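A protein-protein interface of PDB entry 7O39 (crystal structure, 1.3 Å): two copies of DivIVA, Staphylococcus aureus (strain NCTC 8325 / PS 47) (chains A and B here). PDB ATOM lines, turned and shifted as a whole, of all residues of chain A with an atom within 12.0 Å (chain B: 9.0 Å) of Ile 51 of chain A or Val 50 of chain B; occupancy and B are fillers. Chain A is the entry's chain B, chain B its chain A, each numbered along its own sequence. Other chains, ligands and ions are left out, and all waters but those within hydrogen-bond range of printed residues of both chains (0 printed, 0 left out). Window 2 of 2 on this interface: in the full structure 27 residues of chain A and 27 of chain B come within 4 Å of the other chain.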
ATOM      1  N   LYS A  41      -8.645  17.823   5.446  1.00  0.00           N
ATOM      2  CA  LYS A  41      -9.473  18.325   6.542  1.00  0.00           C
ATOM      3  C   LYS A  41      -8.947  19.661   7.062  1.00  0.00           C
ATOM      4  O   LYS A  41      -9.725  20.576   7.359  1.00  0.00           O
ATOM      5  CB  LYS A  41      -9.536  17.284   7.657  1.00  0.00           C
ATOM      6  CG  LYS A  41     -10.391  16.066   7.324  1.00  0.00           C
ATOM      7  CD  LYS A  41     -10.258  14.992   8.394  1.00  0.00           C
ATOM      8  CE  LYS A  41     -11.112  13.775   8.112  1.00  0.00           C
ATOM      9  NZ  LYS A  41     -10.857  12.737   9.150  1.00  0.00           N
ATOM     10  N   GLU A  42      -7.620  19.796   7.162  1.00  0.00           N
ATOM     11  CA  GLU A  42      -7.024  21.080   7.535  1.00  0.00           C
ATOM     12  C   GLU A  42      -7.357  22.155   6.511  1.00  0.00           C
ATOM     13  O   GLU A  42      -7.680  23.293   6.877  1.00  0.00           O
ATOM     14  CB  GLU A  42      -5.502  20.953   7.658  1.00  0.00           C
ATOM     15  CG  GLU A  42      -5.024  20.130   8.850  1.00  0.00           C
ATOM     16  CD  GLU A  42      -3.521  19.836   8.831  1.00  0.00           C
ATOM     17  OE1 GLU A  42      -2.814  20.357   7.944  1.00  0.00           O
ATOM     18  OE2 GLU A  42      -3.054  19.076   9.706  1.00  0.00           O
ATOM     19  N   ASP A  43      -7.267  21.811   5.224  1.00  0.00           N
ATOM     20  CA  ASP A  43      -7.571  22.770   4.165  1.00  0.00           C
ATOM     21  C   ASP A  43      -9.011  23.254   4.283  1.00  0.00           C
ATOM     22  O   ASP A  43      -9.291  24.453   4.121  1.00  0.00           O
ATOM     23  CB  ASP A  43      -7.386  22.115   2.791  1.00  0.00           C
ATOM     24  CG  ASP A  43      -5.942  21.750   2.462  1.00  0.00           C
ATOM     25  OD1 ASP A  43      -4.989  22.190   3.139  1.00  0.00           O
ATOM     26  OD2 ASP A  43      -5.770  20.991   1.481  1.00  0.00           O
ATOM     27  N   LYS A  44      -9.943  22.337   4.567  1.00  0.00           N
ATOM     28  CA  LYS A  44     -11.338  22.730   4.741  1.00  0.00           C
ATOM     29  C   LYS A  44     -11.499  23.698   5.902  1.00  0.00           C
ATOM     30  O   LYS A  44     -12.247  24.677   5.805  1.00  0.00           O
ATOM     31  CB  LYS A  44     -12.193  21.501   5.000  1.00  0.00           C
ATOM     32  CG  LYS A  44     -12.490  20.697   3.781  1.00  0.00           C
ATOM     33  CD  LYS A  44     -13.274  19.436   4.137  1.00  0.00           C
ATOM     34  CE  LYS A  44     -14.596  19.753   4.829  1.00  0.00           C
ATOM     35  NZ  LYS A  44     -15.425  18.517   5.097  1.00  0.00           N
ATOM     36  N   LYS A  45     -10.831  23.423   7.023  1.00  0.00           N
ATOM     37  CA  LYS A  45     -10.939  24.314   8.173  1.00  0.00           C
ATOM     38  C   LYS A  45     -10.412  25.704   7.845  1.00  0.00           C
ATOM     39  O   LYS A  45     -10.962  26.707   8.316  1.00  0.00           O
ATOM     40  CB  LYS A  45     -10.209  23.716   9.378  1.00  0.00           C
ATOM     41  CG  LYS A  45     -10.911  22.521   9.997  1.00  0.00           C
ATOM     42  N   GLN A  46      -9.353  25.793   7.039  1.00  0.00           N
ATOM     43  CA  GLN A  46      -8.839  27.099   6.639  1.00  0.00           C
ATOM     44  C   GLN A  46      -9.847  27.842   5.774  1.00  0.00           C
ATOM     45  O   GLN A  46     -10.029  29.056   5.928  1.00  0.00           O
ATOM     46  CB  GLN A  46      -7.514  26.936   5.895  1.00  0.00           C
ATOM     47  CG  GLN A  46      -6.866  28.258   5.469  1.00  0.00           C
ATOM     48  CD  GLN A  46      -6.746  29.261   6.611  1.00  0.00           C
ATOM     49  OE1 GLN A  46      -6.241  28.936   7.686  1.00  0.00           O
ATOM     50  NE2 GLN A  46      -7.210  30.489   6.377  1.00  0.00           N
ATOM     51  N   LEU A  47     -10.510  27.140   4.857  1.00  0.00           N
ATOM     52  CA  LEU A  47     -11.511  27.787   4.018  1.00  0.00           C
ATOM     53  C   LEU A  47     -12.716  28.219   4.840  1.00  0.00           C
ATOM     54  O   LEU A  47     -13.263  29.308   4.624  1.00  0.00           O
ATOM     55  CB  LEU A  47     -11.925  26.840   2.895  1.00  0.00           C
ATOM     56  CG  LEU A  47     -10.818  26.567   1.874  1.00  0.00           C
ATOM     57  CD1 LEU A  47     -11.180  25.377   1.011  1.00  0.00           C
ATOM     58  CD2 LEU A  47     -10.573  27.793   1.008  1.00  0.00           C
ATOM     59  N   GLU A  48     -13.133  27.391   5.799  1.00  0.00           N
ATOM     60  CA  GLU A  48     -14.221  27.772   6.686  1.00  0.00           C
ATOM     61  C   GLU A  48     -13.850  28.999   7.508  1.00  0.00           C
ATOM     62  O   GLU A  48     -14.709  29.850   7.783  1.00  0.00           O
ATOM     63  CB  GLU A  48     -14.571  26.594   7.594  1.00  0.00           C
ATOM     64  CG  GLU A  48     -15.174  25.414   6.838  1.00  0.00           C
ATOM     65  CD  GLU A  48     -15.180  24.130   7.641  1.00  0.00           C
ATOM     66  OE1 GLU A  48     -14.670  24.132   8.778  1.00  0.00           O
ATOM     67  OE2 GLU A  48     -15.695  23.114   7.129  1.00  0.00           O
ATOM     68  N   LYS A  49     -12.577  29.127   7.883  1.00  0.00           N
ATOM     69  CA  LYS A  49     -12.125  30.310   8.606  1.00  0.00           C
ATOM     70  C   LYS A  49     -12.232  31.560   7.738  1.00  0.00           C
ATOM     71  O   LYS A  49     -12.663  32.618   8.214  1.00  0.00           O
ATOM     72  CB  LYS A  49     -10.689  30.080   9.076  1.00  0.00           C
ATOM     73  CG  LYS A  49     -10.004  31.258   9.738  1.00  0.00           C
ATOM     74  CD  LYS A  49      -8.565  30.886  10.058  1.00  0.00           C
ATOM     75  CE  LYS A  49      -8.015  31.636  11.256  1.00  0.00           C
ATOM     76  NZ  LYS A  49      -6.766  32.357  10.898  1.00  0.00           N
ATOM     77  N   VAL A  50     -11.846  31.462   6.464  1.00  0.00           N
ATOM     78  CA  VAL A  50     -12.001  32.593   5.550  1.00  0.00           C
ATOM     79  C   VAL A  50     -13.461  33.021   5.483  1.00  0.00           C
ATOM     80  O   VAL A  50     -13.777  34.220   5.468  1.00  0.00           O
ATOM     81  CB  VAL A  50     -11.446  32.241   4.156  1.00  0.00           C
ATOM     82  CG1 VAL A  50     -11.838  33.302   3.125  1.00  0.00           C
ATOM     83  CG2 VAL A  50      -9.929  32.080   4.202  1.00  0.00           C
ATOM     84  N   ILE A  51     -14.373  32.047   5.435  1.00  0.00           N
ATOM     85  CA  ILE A  51     -15.795  32.349   5.300  1.00  0.00           C
ATOM     86  C   ILE A  51     -16.334  32.976   6.578  1.00  0.00           C
ATOM     87  O   ILE A  51     -17.111  33.937   6.534  1.00  0.00           O
ATOM     88  CB  ILE A  51     -16.573  31.077   4.904  1.00  0.00           C
ATOM     89  CG1 ILE A  51     -16.243  30.693   3.458  1.00  0.00           C
ATOM     90  CG2 ILE A  51     -18.081  31.280   5.072  1.00  0.00           C
ATOM     91  CD1 ILE A  51     -16.615  29.256   3.094  1.00  0.00           C
ATOM     92  N   GLU A  52     -15.939  32.444   7.736  1.00  0.00           N
ATOM     93  CA  GLU A  52     -16.497  32.924   8.994  1.00  0.00           C
ATOM     94  C   GLU A  52     -16.052  34.346   9.307  1.00  0.00           C
ATOM     95  O   GLU A  52     -16.777  35.085   9.983  1.00  0.00           O
ATOM     96  CB  GLU A  52     -16.101  31.982  10.133  1.00  0.00           C
ATOM     97  N   GLU A  53     -14.873  34.751   8.832  1.00  0.00           N
ATOM     98  CA  GLU A  53     -14.355  36.081   9.129  1.00  0.00           C
ATOM     99  C   GLU A  53     -14.777  37.142   8.121  1.00  0.00           C
ATOM    100  O   GLU A  53     -14.730  38.334   8.449  1.00  0.00           O
ATOM    101  CB  GLU A  53     -12.826  36.066   9.215  1.00  0.00           C
ATOM    102  CG  GLU A  53     -12.272  35.155  10.295  1.00  0.00           C
ATOM    103  CD  GLU A  53     -10.766  35.280  10.449  1.00  0.00           C
ATOM    104  OE1 GLU A  53     -10.281  35.261  11.599  1.00  0.00           O
ATOM    105  OE2 GLU A  53     -10.069  35.403   9.418  1.00  0.00           O
ATOM    106  N   ARG A  54     -15.176  36.755   6.914  1.00  0.00           N
ATOM    107  CA  ARG A  54     -15.622  37.723   5.914  1.00  0.00           C
ATOM    108  C   ARG A  54     -17.057  38.141   6.205  1.00  0.00           C
ATOM    109  O   ARG A  54     -17.318  38.861   7.168  1.00  0.00           O
ATOM    110  CB  ARG A  54     -15.523  37.129   4.506  1.00  0.00           C
ATOM    111  N   ASP B  43     -15.791  18.865  -1.050  1.00  0.00           N
ATOM    112  CA  ASP B  43     -16.120  19.835  -0.009  1.00  0.00           C
ATOM    113  C   ASP B  43     -15.282  21.095  -0.174  1.00  0.00           C
ATOM    114  O   ASP B  43     -15.790  22.218  -0.056  1.00  0.00           O
ATOM    115  CB  ASP B  43     -15.849  19.250   1.384  1.00  0.00           C
ATOM    116  CG  ASP B  43     -16.715  18.058   1.742  1.00  0.00           C
ATOM    117  OD1 ASP B  43     -17.752  17.825   1.098  1.00  0.00           O
ATOM    118  OD2 ASP B  43     -16.340  17.373   2.722  1.00  0.00           O
ATOM    119  N   LYS B  44     -13.977  20.926  -0.412  1.00  0.00           N
ATOM    120  CA  LYS B  44     -13.112  22.084  -0.633  1.00  0.00           C
ATOM    121  C   LYS B  44     -13.579  22.910  -1.819  1.00  0.00           C
ATOM    122  O   LYS B  44     -13.594  24.145  -1.760  1.00  0.00           O
ATOM    123  CB  LYS B  44     -11.681  21.625  -0.882  1.00  0.00           C
ATOM    124  CG  LYS B  44     -10.972  21.181   0.351  1.00  0.00           C
ATOM    125  CD  LYS B  44      -9.592  20.651   0.020  1.00  0.00           C
ATOM    126  CE  LYS B  44      -8.729  21.714  -0.633  1.00  0.00           C
ATOM    127  NZ  LYS B  44      -7.322  21.288  -0.857  1.00  0.00           N
ATOM    128  N   LYS B  45     -13.913  22.249  -2.929  1.00  0.00           N
ATOM    129  CA  LYS B  45     -14.363  22.988  -4.104  1.00  0.00           C
ATOM    130  C   LYS B  45     -15.627  23.783  -3.796  1.00  0.00           C
ATOM    131  O   LYS B  45     -15.784  24.921  -4.258  1.00  0.00           O
ATOM    132  CB  LYS B  45     -14.587  22.028  -5.272  1.00  0.00           C
ATOM    133  CG  LYS B  45     -13.314  21.617  -6.008  1.00  0.00           C
ATOM    134  CD  LYS B  45     -13.562  20.437  -6.957  1.00  0.00           C
ATOM    135  CE  LYS B  45     -12.605  19.262  -6.716  1.00  0.00           C
ATOM    136  NZ  LYS B  45     -13.313  17.943  -6.619  1.00  0.00           N
ATOM    137  N   GLN B  46     -16.537  23.206  -3.007  1.00  0.00           N
ATOM    138  CA  GLN B  46     -17.757  23.921  -2.640  1.00  0.00           C
ATOM    139  C   GLN B  46     -17.434  25.162  -1.821  1.00  0.00           C
ATOM    140  O   GLN B  46     -17.996  26.238  -2.057  1.00  0.00           O
ATOM    141  CB  GLN B  46     -18.701  23.000  -1.856  1.00  0.00           C
ATOM    142  CG  GLN B  46     -20.148  23.524  -1.729  1.00  0.00           C
ATOM    143  CD  GLN B  46     -20.485  24.198  -0.384  1.00  0.00           C
ATOM    144  OE1 GLN B  46     -19.697  24.155   0.564  1.00  0.00           O
ATOM    145  NE2 GLN B  46     -21.679  24.818  -0.307  1.00  0.00           N
ATOM    146  N   LEU B  47     -16.530  25.031  -0.850  1.00  0.00           N
ATOM    147  CA  LEU B  47     -16.161  26.171  -0.021  1.00  0.00           C
ATOM    148  C   LEU B  47     -15.450  27.243  -0.843  1.00  0.00           C
ATOM    149  O   LEU B  47     -15.697  28.445  -0.662  1.00  0.00           O
ATOM    150  CB  LEU B  47     -15.285  25.693   1.137  1.00  0.00           C
ATOM    151  CG  LEU B  47     -15.976  24.765   2.140  1.00  0.00           C
ATOM    152  CD1 LEU B  47     -14.960  24.040   3.019  1.00  0.00           C
ATOM    153  CD2 LEU B  47     -16.968  25.549   2.989  1.00  0.00           C
ATOM    154  N   GLU B  48     -14.559  26.832  -1.751  1.00  0.00           N
ATOM    155  CA  GLU B  48     -13.885  27.797  -2.617  1.00  0.00           C
ATOM    156  C   GLU B  48     -14.894  28.562  -3.468  1.00  0.00           C
ATOM    157  O   GLU B  48     -14.734  29.767  -3.712  1.00  0.00           O
ATOM    158  CB  GLU B  48     -12.867  27.074  -3.504  1.00  0.00           C
ATOM    159  CG  GLU B  48     -11.631  26.599  -2.746  1.00  0.00           C
ATOM    160  CD  GLU B  48     -10.769  25.618  -3.533  1.00  0.00           C
ATOM    161  OE1 GLU B  48     -11.203  25.141  -4.603  1.00  0.00           O
ATOM    162  OE2 GLU B  48      -9.647  25.327  -3.072  1.00  0.00           O
ATOM    163  N   LYS B  49     -15.947  27.885  -3.928  1.00  0.00           N
ATOM    164  CA  LYS B  49     -16.957  28.563  -4.736  1.00  0.00           C
ATOM    165  C   LYS B  49     -17.744  29.567  -3.904  1.00  0.00           C
ATOM    166  O   LYS B  49     -18.070  30.655  -4.387  1.00  0.00           O
ATOM    167  CB  LYS B  49     -17.890  27.542  -5.386  1.00  0.00           C
ATOM    168  CG  LYS B  49     -17.246  26.738  -6.501  1.00  0.00           C
ATOM    169  N   VAL B  50     -18.060  29.225  -2.652  1.00  0.00           N
ATOM    170  CA  VAL B  50     -18.730  30.184  -1.773  1.00  0.00           C
ATOM    171  C   VAL B  50     -17.871  31.428  -1.607  1.00  0.00           C
ATOM    172  O   VAL B  50     -18.373  32.559  -1.643  1.00  0.00           O
ATOM    173  CB  VAL B  50     -19.052  29.519  -0.421  1.00  0.00           C
ATOM    174  CG1 VAL B  50     -19.456  30.550   0.626  1.00  0.00           C
ATOM    175  CG2 VAL B  50     -20.132  28.469  -0.605  1.00  0.00           C
ATOM    176  N   ILE B  51     -16.562  31.243  -1.435  1.00  0.00           N
ATOM    177  CA  ILE B  51     -15.660  32.379  -1.279  1.00  0.00           C
ATOM    178  C   ILE B  51     -15.594  33.193  -2.565  1.00  0.00           C
ATOM    179  O   ILE B  51     -15.647  34.434  -2.536  1.00  0.00           O
ATOM    180  CB  ILE B  51     -14.270  31.888  -0.827  1.00  0.00           C
ATOM    181  CG1 ILE B  51     -14.367  31.293   0.580  1.00  0.00           C
ATOM    182  CG2 ILE B  51     -13.254  33.031  -0.857  1.00  0.00           C
ATOM    183  CD1 ILE B  51     -13.199  30.415   0.962  1.00  0.00           C
ATOM    184  N   GLU B  52     -15.497  32.524  -3.714  1.00  0.00           N
ATOM    185  CA  GLU B  52     -15.378  33.252  -4.973  1.00  0.00           C
ATOM    186  C   GLU B  52     -16.645  34.043  -5.272  1.00  0.00           C
ATOM    187  O   GLU B  52     -16.579  35.157  -5.808  1.00  0.00           O
ATOM    188  CB  GLU B  52     -15.068  32.285  -6.115  1.00  0.00           C
ATOM    189  N   GLU B  53     -17.808  33.494  -4.924  1.00  0.00           N
ATOM    190  CA  GLU B  53     -19.054  34.201  -5.198  1.00  0.00           C
ATOM    191  C   GLU B  53     -19.239  35.390  -4.267  1.00  0.00           C
ATOM    192  O   GLU B  53     -19.950  36.341  -4.616  1.00  0.00           O
ATOM    193  CB  GLU B  53     -20.232  33.229  -5.138  1.00  0.00           C
ATOM    194  CG  GLU B  53     -20.108  32.111  -6.168  1.00  0.00           C
ATOM    195  CD  GLU B  53     -21.057  30.957  -5.925  1.00  0.00           C
ATOM    196  OE1 GLU B  53     -21.316  30.194  -6.883  1.00  0.00           O
ATOM    197  OE2 GLU B  53     -21.538  30.807  -4.782  1.00  0.00           O
ATOM    198  N   ARG B  54     -18.604  35.369  -3.099  1.00  0.00           N
ATOM    199  CA  ARG B  54     -18.605  36.509  -2.184  1.00  0.00           C
ATOM    200  C   ARG B  54     -19.994  36.761  -1.606  1.00  0.00           C
ATOM    201  O   ARG B  54     -21.008  36.503  -2.254  1.00  0.00           O
ATOM    202  CB  ARG B  54     -18.087  37.773  -2.884  1.00  0.00           C
ATOM    203  CG  ARG B  54     -16.621  37.703  -3.292  1.00  0.00           C
ATOM    204  CD  ARG B  54     -16.274  38.755  -4.342  1.00  0.00           C
ATOM    205  NE  ARG B  54     -16.380  38.241  -5.709  1.00  0.00           N
ATOM    206  CZ  ARG B  54     -17.409  38.454  -6.529  1.00  0.00           C
ATOM    207  NH1 ARG B  54     -18.455  39.177  -6.141  1.00  0.00           N
ATOM    208  NH2 ARG B  54     -17.394  37.937  -7.750  1.00  0.00           N
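Hydrophobic or aromatic side chains of chain B that line the printed part of chain A: Leu 47, Val 50 and Ile 51. Of the 14 printed residues of chain A, 5 touch a printed residue of chain B. Printed residues of chain A that touch a printed residue of chain B: Asp 43, Lys 44, Leu 47, Val 50 and Ile 51. Along chain A the printed residues that touch a printed residue of chain B span positions 43 to 51. Among the printed residues, 12 pairs touch across the chains.
Of the printed residues of chain B, Asp 43 of chain A touches Lys 44 (2.8 Å). Of the printed residues of chain B, Lys 44 of chain A touches Asp 43, Lys 44 and Leu 47. Glu 48 of chain A touches none of the printed residues of chain B. Of chain B, only Leu 47 (3.7 Å), Val 50 (3.98 Å) and Ile 51 (3.5 Å) come within 4 Å of Ile 51 of chain A. Glu 52 of chain A touches none of the printed residues of chain B. Of the printed residues of chain A, Asp 43 of chain B touches Lys 44 (2.8 Å). No residue of chain A comes within 4 Å of Gln 46 of chain B. Leu 47 of chain B touches just these residues of chain A: Lys 44 (3.9 Å), Leu 47 (3.96 Å) and Ile 51 (3.7 Å). Of the printed residues of chain A, Glu 48 of chain B touches Leu 47 (3.98 Å). No residue of chain A comes within 4 Å of Lys 49 of chain B. Val 50 of chain B touches just one residue of chain A: Ile 51. Ile 51 of chain B touches just these residues of chain A: Leu 47, Val 50 and Ile 51. Glu 52 of chain B touches none of the printed residues of chain A. No residue of chain A comes within 4 Å of Glu 53 of chain B. The nearest residue of chain A that does not touch Val 50 of chain B is Leu 47 of chain A (7.5 Å).
Among the printed residues, merely in contact across the chains: Lys 44 of chain A with Lys 44 of chain B (3.8 Å), Lys 44 of chain A with Leu 47 of chain B (3.9 Å), Leu 47 of chain A with Lys 44 of chain B (3.9 Å), Leu 47 of chain A with Leu 47 of chain B (3.96 Å), Leu 47 of chain A with Glu 48 of chain B (3.98 Å), Leu 47 of chain A with Ile 51 of chain B (3.7 Å), Val 50 of chain A with Ile 51 of chain B (3.9 Å), Ile 51 of chain A with Leu 47 of chain B (3.7 Å), Ile 51 of chain A with Val 50 of chain B (3.98 Å) and Ile 51 of chain A with Ile 51 of chain B (3.5 Å).
Lys 44 of chain A touches Leu 47 of chain B, and with the chains exchanged Leu 47 of chain A touches Lys 44 of chain B. Leu 47 of chain B touches its own counterpart, Leu 47 of chain A. Leu 47 of chain A touches Glu 48 of chain B, but with the chains exchanged Glu 48 of chain A does not touch Leu 47 of chain B (4.1 Å). Leu 47 of chain A touches Ile 51 of chain B, and with the chains exchanged Ile 51 of chain A touches Leu 47 of chain B. Of the 12 pairs that touch across the chains among the printed residues, 11 have their exchanged pair printed and touching as well.
The side-chain carboxylate (OD2) of Asp 43 of chain A lies within salt-bridge range of the side-chain amino group (NZ) of Lys 44 of chain B (2.8 Å). The side-chain carboxylate (OD2) of Asp 43 of chain B lies within salt-bridge range of the side-chain amino group (NZ) of Lys 44 of chain A (2.8 Å).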
